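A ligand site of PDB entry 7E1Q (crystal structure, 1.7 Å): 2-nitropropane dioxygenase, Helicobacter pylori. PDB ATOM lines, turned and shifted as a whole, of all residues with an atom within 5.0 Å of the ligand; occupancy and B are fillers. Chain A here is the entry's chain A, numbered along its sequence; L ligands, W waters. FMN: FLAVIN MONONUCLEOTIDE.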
ATOM      1  N   GLY A  31     -26.960 -22.099  21.836  1.00  0.00           N
ATOM      2  CA  GLY A  31     -28.179 -21.873  21.057  1.00  0.00           C
ATOM      3  C   GLY A  31     -27.898 -21.809  19.554  1.00  0.00           C
ATOM      4  O   GLY A  31     -26.904 -21.239  19.103  1.00  0.00           O
ATOM      5  N   GLY A  32     -28.821 -22.386  18.784  1.00  0.00           N
ATOM      6  CA  GLY A  32     -28.684 -22.316  17.339  1.00  0.00           C
ATOM      7  C   GLY A  32     -28.749 -20.871  16.858  1.00  0.00           C
ATOM      8  O   GLY A  32     -29.481 -20.050  17.400  1.00  0.00           O
ATOM      9  N   MET A  33     -27.978 -20.577  15.804  1.00  0.00           N
ATOM     10  CA  MET A  33     -27.836 -19.218  15.286  1.00  0.00           C
ATOM     11  C   MET A  33     -27.753 -19.299  13.766  1.00  0.00           C
ATOM     12  O   MET A  33     -26.786 -19.848  13.220  1.00  0.00           O
ATOM     13  CB  MET A  33     -26.563 -18.625  15.902  1.00  0.00           C
ATOM     14  CG  MET A  33     -26.777 -18.223  17.339  1.00  0.00           C
ATOM     15  SD  MET A  33     -25.429 -17.254  18.003  1.00  0.00           S
ATOM     16  CE  MET A  33     -24.204 -18.580  18.186  1.00  0.00           C
ATOM     17  N   GLY A  34     -28.763 -18.781  13.066  1.00  0.00           N
ATOM     18  CA  GLY A  34     -28.720 -18.727  11.604  1.00  0.00           C
ATOM     19  C   GLY A  34     -28.469 -17.317  11.087  1.00  0.00           C
ATOM     20  O   GLY A  34     -28.664 -16.372  11.861  1.00  0.00           O
ATOM     21  N   ILE A  37     -24.111 -19.146  11.317  1.00  0.00           N
ATOM     22  CA  ILE A  37     -23.393 -18.724  12.505  1.00  0.00           C
ATOM     23  C   ILE A  37     -22.972 -19.930  13.349  1.00  0.00           C
ATOM     24  O   ILE A  37     -21.799 -20.055  13.722  1.00  0.00           O
ATOM     25  CB  ILE A  37     -24.271 -17.728  13.300  1.00  0.00           C
ATOM     26  CG1 ILE A  37     -24.656 -16.536  12.405  1.00  0.00           C
ATOM     27  CG2 ILE A  37     -23.553 -17.271  14.559  1.00  0.00           C
ATOM     28  CD1 ILE A  37     -25.567 -15.515  13.065  1.00  0.00           C
ATOM     29  N   SER A  56     -27.525 -24.864  13.200  1.00  0.00           N
ATOM     30  CA  SER A  56     -28.675 -24.235  12.560  1.00  0.00           C
ATOM     31  C   SER A  56     -28.927 -24.838  11.183  1.00  0.00           C
ATOM     32  O   SER A  56     -28.017 -24.905  10.358  1.00  0.00           O
ATOM     33  CB  SER A  56     -28.454 -22.729  12.434  1.00  0.00           C
ATOM     34  OG  SER A  56     -29.440 -22.167  11.593  1.00  0.00           O
ATOM     35  N   ASN A 108     -31.323 -26.904  14.869  1.00  0.00           N
ATOM     36  CA  ASN A 108     -32.306 -25.864  15.130  1.00  0.00           C
ATOM     37  C   ASN A 108     -33.058 -25.551  13.849  1.00  0.00           C
ATOM     38  O   ASN A 108     -32.437 -25.221  12.821  1.00  0.00           O
ATOM     39  CB  ASN A 108     -31.625 -24.605  15.657  1.00  0.00           C
ATOM     40  CG  ASN A 108     -32.623 -23.510  15.944  1.00  0.00           C
ATOM     41  OD1 ASN A 108     -33.212 -22.926  15.036  1.00  0.00           O
ATOM     42  ND2 ASN A 108     -32.828 -23.241  17.226  1.00  0.00           N
ATOM     43  N   LEU A 110     -36.447 -23.252  12.631  1.00  0.00           N
ATOM     44  CA  LEU A 110     -37.596 -22.397  12.904  1.00  0.00           C
ATOM     45  C   LEU A 110     -38.867 -23.031  12.351  1.00  0.00           C
ATOM     46  O   LEU A 110     -38.897 -23.525  11.219  1.00  0.00           O
ATOM     47  CB  LEU A 110     -37.398 -21.007  12.299  1.00  0.00           C
ATOM     48  CG  LEU A 110     -36.560 -19.966  13.030  1.00  0.00           C
ATOM     49  CD1 LEU A 110     -35.091 -20.299  13.002  1.00  0.00           C
ATOM     50  CD2 LEU A 110     -36.804 -18.590  12.389  1.00  0.00           C
ATOM     51  N   GLY A 134     -38.378 -23.115  17.475  1.00  0.00           N
ATOM     52  CA  GLY A 134     -39.167 -21.968  17.912  1.00  0.00           C
ATOM     53  C   GLY A 134     -39.816 -21.259  16.730  1.00  0.00           C
ATOM     54  O   GLY A 134     -40.118 -21.909  15.727  1.00  0.00           O
ATOM     55  N   ILE A 156     -39.283 -24.444  21.601  1.00  0.00           N
ATOM     56  CA  ILE A 156     -38.974 -23.196  22.307  1.00  0.00           C
ATOM     57  C   ILE A 156     -40.282 -22.472  22.580  1.00  0.00           C
ATOM     58  O   ILE A 156     -41.083 -22.255  21.650  1.00  0.00           O
ATOM     59  CB  ILE A 156     -38.026 -22.295  21.490  1.00  0.00           C
ATOM     60  CG1 ILE A 156     -36.741 -23.033  21.115  1.00  0.00           C
ATOM     61  CG2 ILE A 156     -37.696 -21.007  22.285  1.00  0.00           C
ATOM     62  CD1 ILE A 156     -35.829 -22.214  20.172  1.00  0.00           C
ATOM     63  N   GLU A 184     -37.472 -19.126  26.192  1.00  0.00           N
ATOM     64  CA  GLU A 184     -36.650 -18.065  25.631  1.00  0.00           C
ATOM     65  C   GLU A 184     -37.215 -16.714  26.082  1.00  0.00           C
ATOM     66  O   GLU A 184     -38.320 -16.325  25.662  1.00  0.00           O
ATOM     67  CB  GLU A 184     -36.580 -18.164  24.110  1.00  0.00           C
ATOM     68  CG  GLU A 184     -35.321 -17.539  23.549  1.00  0.00           C
ATOM     69  CD  GLU A 184     -35.176 -17.653  22.042  1.00  0.00           C
ATOM     70  OE1 GLU A 184     -34.038 -17.515  21.574  1.00  0.00           O
ATOM     71  OE2 GLU A 184     -36.183 -17.894  21.320  1.00  0.00           O
ATOM     72  N   LEU A 187     -34.556 -11.120  26.452  1.00  0.00           N
ATOM     73  CA  LEU A 187     -33.221 -10.602  26.208  1.00  0.00           C
ATOM     74  C   LEU A 187     -32.471 -11.402  25.136  1.00  0.00           C
ATOM     75  O   LEU A 187     -31.323 -11.079  24.832  1.00  0.00           O
ATOM     76  CB  LEU A 187     -32.403 -10.592  27.506  1.00  0.00           C
ATOM     77  CG  LEU A 187     -33.026  -9.706  28.605  1.00  0.00           C
ATOM     78  CD1 LEU A 187     -32.208  -9.814  29.877  1.00  0.00           C
ATOM     79  CD2 LEU A 187     -33.129  -8.245  28.164  1.00  0.00           C
ATOM     80  N   SER A 188     -33.136 -12.389  24.531  1.00  0.00           N
ATOM     81  CA  SER A 188     -32.509 -13.265  23.559  1.00  0.00           C
ATOM     82  C   SER A 188     -32.158 -12.514  22.277  1.00  0.00           C
ATOM     83  O   SER A 188     -32.673 -11.443  21.992  1.00  0.00           O
ATOM     84  CB  SER A 188     -33.438 -14.424  23.224  1.00  0.00           C
ATOM     85  OG  SER A 188     -34.631 -13.921  22.668  1.00  0.00           O
ATOM     86  N   GLY A 189     -31.266 -13.133  21.469  1.00  0.00           N
ATOM     87  CA  GLY A 189     -30.993 -12.614  20.150  1.00  0.00           C
ATOM     88  C   GLY A 189     -31.949 -13.186  19.128  1.00  0.00           C
ATOM     89  O   GLY A 189     -32.640 -14.172  19.380  1.00  0.00           O
ATOM     90  N   GLY A 190     -32.026 -12.524  17.966  1.00  0.00           N
ATOM     91  CA  GLY A 190     -32.945 -13.035  16.950  1.00  0.00           C
ATOM     92  C   GLY A 190     -34.401 -12.789  17.322  1.00  0.00           C
ATOM     93  O   GLY A 190     -34.727 -11.839  18.026  1.00  0.00           O
ATOM     94  N   ALA A 228     -33.295 -19.600  28.613  1.00  0.00           N
ATOM     95  CA  ALA A 228     -32.499 -18.917  27.599  1.00  0.00           C
ATOM     96  C   ALA A 228     -32.852 -17.438  27.541  1.00  0.00           C
ATOM     97  O   ALA A 228     -34.020 -17.056  27.723  1.00  0.00           O
ATOM     98  CB  ALA A 228     -32.695 -19.547  26.207  1.00  0.00           C
ATOM     99  N   GLY A 229     -31.848 -16.616  27.258  1.00  0.00           N
ATOM    100  CA  GLY A 229     -32.041 -15.191  27.023  1.00  0.00           C
ATOM    101  C   GLY A 229     -31.421 -14.337  28.107  1.00  0.00           C
ATOM    102  O   GLY A 229     -31.981 -14.212  29.203  1.00  0.00           O
ATOM    103  N   GLY A 230     -30.242 -13.778  27.827  1.00  0.00           N
ATOM    104  CA  GLY A 230     -29.591 -12.891  28.777  1.00  0.00           C
ATOM    105  C   GLY A 230     -28.720 -13.576  29.809  1.00  0.00           C
ATOM    106  O   GLY A 230     -28.262 -12.913  30.745  1.00  0.00           O
ATOM    107  N   ILE A 231     -28.483 -14.875  29.658  1.00  0.00           N
ATOM    108  CA  ILE A 231     -27.623 -15.622  30.575  1.00  0.00           C
ATOM    109  C   ILE A 231     -26.190 -15.425  30.107  1.00  0.00           C
ATOM    110  O   ILE A 231     -25.834 -15.797  28.983  1.00  0.00           O
ATOM    111  CB  ILE A 231     -28.021 -17.101  30.603  1.00  0.00           C
ATOM    112  CG1 ILE A 231     -29.470 -17.221  31.059  1.00  0.00           C
ATOM    113  CG2 ILE A 231     -27.067 -17.904  31.511  1.00  0.00           C
ATOM    114  CD1 ILE A 231     -30.074 -18.596  30.805  1.00  0.00           C
ATOM    115  N   GLN A 249     -29.641 -22.392  27.875  1.00  0.00           N
ATOM    116  CA  GLN A 249     -29.191 -22.220  26.500  1.00  0.00           C
ATOM    117  C   GLN A 249     -28.625 -20.802  26.365  1.00  0.00           C
ATOM    118  O   GLN A 249     -29.272 -19.833  26.779  1.00  0.00           O
ATOM    119  CB  GLN A 249     -30.331 -22.438  25.495  1.00  0.00           C
ATOM    120  CG  GLN A 249     -29.932 -22.128  24.045  1.00  0.00           C
ATOM    121  CD  GLN A 249     -30.948 -22.620  23.041  1.00  0.00           C
ATOM    122  OE1 GLN A 249     -30.903 -23.775  22.613  1.00  0.00           O
ATOM    123  NE2 GLN A 249     -31.876 -21.746  22.653  1.00  0.00           N
ATOM    124  N   MET A 250     -27.426 -20.712  25.813  1.00  0.00           N
ATOM    125  CA  MET A 250     -26.689 -19.459  25.694  1.00  0.00           C
ATOM    126  C   MET A 250     -26.199 -19.330  24.260  1.00  0.00           C
ATOM    127  O   MET A 250     -25.737 -20.311  23.680  1.00  0.00           O
ATOM    128  CB  MET A 250     -25.508 -19.442  26.668  1.00  0.00           C
ATOM    129  CG  MET A 250     -25.933 -19.537  28.128  1.00  0.00           C
ATOM    130  SD  MET A 250     -24.508 -19.796  29.216  1.00  0.00           S
ATOM    131  CE  MET A 250     -23.608 -18.252  28.995  1.00  0.00           C
ATOM    132  N   ALA A 251     -26.340 -18.132  23.686  1.00  0.00           N
ATOM    133  CA  ALA A 251     -25.904 -17.932  22.309  1.00  0.00           C
ATOM    134  C   ALA A 251     -24.909 -16.773  22.184  1.00  0.00           C
ATOM    135  O   ALA A 251     -23.843 -16.939  21.589  1.00  0.00           O
ATOM    136  CB  ALA A 251     -27.103 -17.699  21.393  1.00  0.00           C
ATOM    137  N   THR A 252     -25.236 -15.612  22.759  1.00  0.00           N
ATOM    138  CA  THR A 252     -24.365 -14.437  22.577  1.00  0.00           C
ATOM    139  C   THR A 252     -22.933 -14.715  23.025  1.00  0.00           C
ATOM    140  O   THR A 252     -21.979 -14.302  22.349  1.00  0.00           O
ATOM    141  CB  THR A 252     -24.948 -13.211  23.296  1.00  0.00           C
ATOM    142  OG1 THR A 252     -26.196 -12.855  22.686  1.00  0.00           O
ATOM    143  CG2 THR A 252     -24.012 -11.996  23.194  1.00  0.00           C
ATOM    144  N   LEU A 255     -21.470 -16.570  20.198  1.00  0.00           N
ATOM    145  CA  LEU A 255     -21.273 -15.637  19.098  1.00  0.00           C
ATOM    146  C   LEU A 255     -19.941 -14.918  19.242  1.00  0.00           C
ATOM    147  O   LEU A 255     -19.349 -14.477  18.254  1.00  0.00           O
ATOM    148  CB  LEU A 255     -22.436 -14.640  19.072  1.00  0.00           C
ATOM    149  CG  LEU A 255     -22.625 -13.736  17.849  1.00  0.00           C
ATOM    150  CD1 LEU A 255     -22.912 -14.545  16.600  1.00  0.00           C
ATOM    151  CD2 LEU A 255     -23.729 -12.723  18.127  1.00  0.00           C
ATOM    152  N   TYR A 265     -18.528 -11.854  12.836  1.00  0.00           N
ATOM    153  CA  TYR A 265     -18.904 -11.432  14.182  1.00  0.00           C
ATOM    154  C   TYR A 265     -17.683 -11.172  15.057  1.00  0.00           C
ATOM    155  O   TYR A 265     -17.779 -10.381  15.997  1.00  0.00           O
ATOM    156  CB  TYR A 265     -19.832 -12.467  14.831  1.00  0.00           C
ATOM    157  CG  TYR A 265     -21.276 -12.301  14.393  1.00  0.00           C
ATOM    158  CD1 TYR A 265     -22.116 -11.404  15.044  1.00  0.00           C
ATOM    159  CD2 TYR A 265     -21.789 -13.011  13.301  1.00  0.00           C
ATOM    160  CE1 TYR A 265     -23.434 -11.236  14.645  1.00  0.00           C
ATOM    161  CE2 TYR A 265     -23.103 -12.852  12.899  1.00  0.00           C
ATOM    162  CZ  TYR A 265     -23.923 -11.973  13.564  1.00  0.00           C
ATOM    163  OH  TYR A 265     -25.248 -11.816  13.153  1.00  0.00           O
ATOM    164  N   PHE A 348     -27.615 -10.125  13.998  1.00  0.00           N
ATOM    165  CA  PHE A 348     -28.439 -10.313  15.188  1.00  0.00           C
ATOM    166  C   PHE A 348     -27.548 -10.323  16.438  1.00  0.00           C
ATOM    167  O   PHE A 348     -26.334 -10.535  16.336  1.00  0.00           O
ATOM    168  CB  PHE A 348     -29.218 -11.645  15.121  1.00  0.00           C
ATOM    169  CG  PHE A 348     -30.434 -11.624  14.234  1.00  0.00           C
ATOM    170  CD1 PHE A 348     -30.974 -10.443  13.739  1.00  0.00           C
ATOM    171  CD2 PHE A 348     -31.061 -12.827  13.908  1.00  0.00           C
ATOM    172  CE1 PHE A 348     -32.117 -10.467  12.923  1.00  0.00           C
ATOM    173  CE2 PHE A 348     -32.197 -12.864  13.108  1.00  0.00           C
ATOM    174  CZ  PHE A 348     -32.715 -11.683  12.609  1.00  0.00           C
ATOM    175  N   THR A 349     -28.148 -10.087  17.597  1.00  0.00           N
ATOM    176  CA  THR A 349     -27.409 -10.149  18.863  1.00  0.00           C
ATOM    177  C   THR A 349     -28.416 -10.293  20.003  1.00  0.00           C
ATOM    178  O   THR A 349     -29.548  -9.821  19.907  1.00  0.00           O
ATOM    179  CB  THR A 349     -26.560  -8.891  19.089  1.00  0.00           C
ATOM    180  OG1 THR A 349     -25.893  -8.964  20.355  1.00  0.00           O
ATOM    181  CG2 THR A 349     -27.425  -7.629  19.107  1.00  0.00           C
ATOM    182  N   GLY A 350     -27.985 -10.914  21.088  1.00  0.00           N
ATOM    183  CA  GLY A 350     -28.734 -10.795  22.322  1.00  0.00           C
ATOM    184  C   GLY A 350     -28.568  -9.408  22.918  1.00  0.00           C
ATOM    185  O   GLY A 350     -27.709  -8.628  22.507  1.00  0.00           O
ATOM    186  N   ASN A 352     -27.172  -8.732  25.589  1.00  0.00           N
ATOM    187  CA  ASN A 352     -25.850  -8.627  26.192  1.00  0.00           C
ATOM    188  C   ASN A 352     -24.712  -8.482  25.175  1.00  0.00           C
ATOM    189  O   ASN A 352     -23.545  -8.497  25.593  1.00  0.00           O
ATOM    190  CB  ASN A 352     -25.562  -9.851  27.078  1.00  0.00           C
ATOM    191  CG  ASN A 352     -26.242  -9.760  28.438  1.00  0.00           C
ATOM    192  OD1 ASN A 352     -26.411  -8.677  28.987  1.00  0.00           O
ATOM    193  ND2 ASN A 352     -26.626 -10.920  28.981  1.00  0.00           N
HETATM  194  N1  FMN L   1     -32.786 -18.938  17.872  1.00  0.00           N
HETATM  195  C2  FMN L   1     -33.372 -19.911  17.079  1.00  0.00           C
HETATM  196  O2  FMN L   1     -34.219 -20.682  17.553  1.00  0.00           O
HETATM  197  N3  FMN L   1     -33.012 -19.983  15.729  1.00  0.00           N
HETATM  198  C4  FMN L   1     -32.078 -19.080  15.185  1.00  0.00           C
HETATM  199  O4  FMN L   1     -31.788 -19.189  13.995  1.00  0.00           O
HETATM  200  C4A FMN L   1     -31.493 -18.103  16.000  1.00  0.00           C
HETATM  201  N5  FMN L   1     -30.586 -17.229  15.506  1.00  0.00           N
HETATM  202  C5A FMN L   1     -29.881 -16.445  16.351  1.00  0.00           C
HETATM  203  C6  FMN L   1     -28.802 -15.668  15.878  1.00  0.00           C
HETATM  204  C7  FMN L   1     -28.047 -14.869  16.747  1.00  0.00           C
HETATM  205  C7M FMN L   1     -26.955 -14.096  16.271  1.00  0.00           C
HETATM  206  C8  FMN L   1     -28.374 -14.840  18.103  1.00  0.00           C
HETATM  207  C8M FMN L   1     -27.631 -14.058  19.013  1.00  0.00           C
HETATM  208  C9  FMN L   1     -29.441 -15.597  18.568  1.00  0.00           C
HETATM  209  C9A FMN L   1     -30.205 -16.401  17.699  1.00  0.00           C
HETATM  210  N10 FMN L   1     -31.241 -17.154  18.159  1.00  0.00           N
HETATM  211  C10 FMN L   1     -31.841 -18.033  17.337  1.00  0.00           C
HETATM  212  C1' FMN L   1     -31.563 -17.234  19.614  1.00  0.00           C
HETATM  213  C2' FMN L   1     -30.495 -18.109  20.371  1.00  0.00           C
HETATM  214  O2' FMN L   1     -30.528 -19.474  19.911  1.00  0.00           O
HETATM  215  C3' FMN L   1     -30.640 -18.107  21.906  1.00  0.00           C
HETATM  216  O3' FMN L   1     -31.830 -18.780  22.318  1.00  0.00           O
HETATM  217  C4' FMN L   1     -30.605 -16.695  22.553  1.00  0.00           C
HETATM  218  O4' FMN L   1     -29.800 -15.759  21.852  1.00  0.00           O
HETATM  219  C5' FMN L   1     -30.063 -16.877  23.984  1.00  0.00           C
HETATM  220  O5' FMN L   1     -29.822 -15.593  24.617  1.00  0.00           O
HETATM  221  P   FMN L   1     -28.344 -15.052  24.779  1.00  0.00           P
HETATM  222  O1P FMN L   1     -27.565 -16.183  25.366  1.00  0.00           O
HETATM  223  O2P FMN L   1     -27.958 -14.753  23.381  1.00  0.00           O
HETATM  224  O3P FMN L   1     -28.472 -13.886  25.682  1.00  0.00           O
HETATM  225  O   HOH W   1     -36.014 -22.298  16.069  1.00  0.00           O
HETATM  226  O   HOH W   2     -28.611 -11.209  25.900  1.00  0.00           O
HETATM  227  O   HOH W   3     -34.593 -16.376  18.940  1.00  0.00           O
HETATM  228  O   HOH W   4     -24.923 -16.073  26.178  1.00  0.00           O
HETATM  229  O   HOH W   5     -29.031 -17.118  27.414  1.00  0.00           O
HETATM  230  O   HOH W   6     -32.745 -21.098  19.907  1.00  0.00           O
HETATM  231  O   HOH W   7     -26.362 -13.310  27.379  1.00  0.00           O
HETATM  232  O   HOH W   8     -31.685 -21.772  13.004  1.00  0.00           O
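The side-chain amide nitrogen (ND2) of Asn 108 sits at hydrogen-bond distance from an oxygen (O2) of the ligand (2.9 Å). O4' of the ligand lies within hydrogen-bond range of N of Gly 189 (3.0 Å). An oxygen (O2P) of the ligand sits at hydrogen-bond distance from the backbone NH of Thr 252, at 2.9 Å. N of Gly 34 sits at hydrogen-bond distance from O4 of the ligand, at 3.2 Å. An oxygen (O3P) of the ligand is in hydrogen-bond range of the backbone NH (N) of Gly 230 (2.8 Å). The backbone NH (N) of Gly 229 lies close to an oxygen (O5') of the ligand, 3.5 Å away. An oxygen (O2P) of the ligand lies within hydrogen-bond range of the side-chain hydroxyl of Thr 252, at 2.7 Å. The side-chain amide nitrogen (NE2) of Gln 249 is in hydrogen-bond range of an oxygen (O3') of the ligand, 3.0 Å away. OE1 of Glu 184 lies within hydrogen-bond range of O3' of the ligand (2.7 Å). The backbone NH (N) of Ala 251 is in hydrogen-bond range of an oxygen (O1P) of the ligand (2.8 Å). O of Gly 32 is in hydrogen-bond range of O2' of the ligand (2.8 Å).
Water W5 lies within hydrogen-bond range of O1P of the ligand, O of Gln 249, N of Gly 229 and N of Ile 231. Water W6 lies within hydrogen-bond range of an oxygen (O2') of the ligand, the side-chain amide nitrogen (NE2) of Gln 249 and the side-chain amide nitrogen (ND2) of Asn 108. Water W4 lies within hydrogen-bond range of an oxygen (O1P) of the ligand (2.8 Å), the backbone carbonyl oxygen (O) of Ile 231 (3.0 Å) and the backbone NH (N) of Thr 252 (3.5 Å). Water W7 lies within hydrogen-bond range of O3P of the ligand (2.8 Å), ND2 of Asn 352 (2.9 Å) and O of Ile 231 (3.0 Å). Water W8 lies within hydrogen-bond range of OG of Ser 56 (2.7 Å), O4 of the ligand (2.8 Å) and OD1 of Asn 108 (2.8 Å). Water W1 lies within hydrogen-bond range of O2 of the ligand (2.8 Å), N of Gly 134 (2.9 Å) and OD1 of Asn 108 (3.1 Å).
C of Gly 31 touches O2' of the ligand (3.5 Å). CA of Met 33 touches N5 of the ligand, 3.4 Å away. CD1 of Ile 37 touches C7M of the ligand, 3.8 Å away. Leu 110 touches the ligand (CD1 to N3, 3.4 Å). Ile 156 touches the ligand. CB of Ser 188 touches C4' of the ligand, at 3.7 Å. Met 250 touches the ligand. Leu 255 touches the ligand (CD2 to C7M, 3.97 Å). Phe 348 touches the ligand. Thr 349 touches the ligand (CA to C8M, 3.9 Å). Gly 350 touches the ligand. Within 4 Å of the ligand: Gly 31, Gly 32, Met 33, Gly 34, Ile 37, Asn 108, Leu 110, Ile 156, Glu 184, Ser 188, Gly 189, Gly 229, Gly 230, Gln 249, Met 250, Ala 251, Thr 252, Leu 255, Phe 348, Thr 349 and Gly 350.
The side-chain hydroxyl (OG1) of Thr 252 lies within hydrogen-bond range of the backbone NH (N) of Gly 350 (3.1 Å). The backbone NH of Gly 31 lies within hydrogen-bond range of the backbone carbonyl oxygen of Met 250 (2.8 Å). The backbone NH (N) of Phe 348 is in hydrogen-bond range of the side-chain hydroxyl (OH) of Tyr 265 (3.0 Å). The side-chain amide nitrogen of Asn 352 lies within hydrogen-bond range of the backbone carbonyl oxygen of Gly 230.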
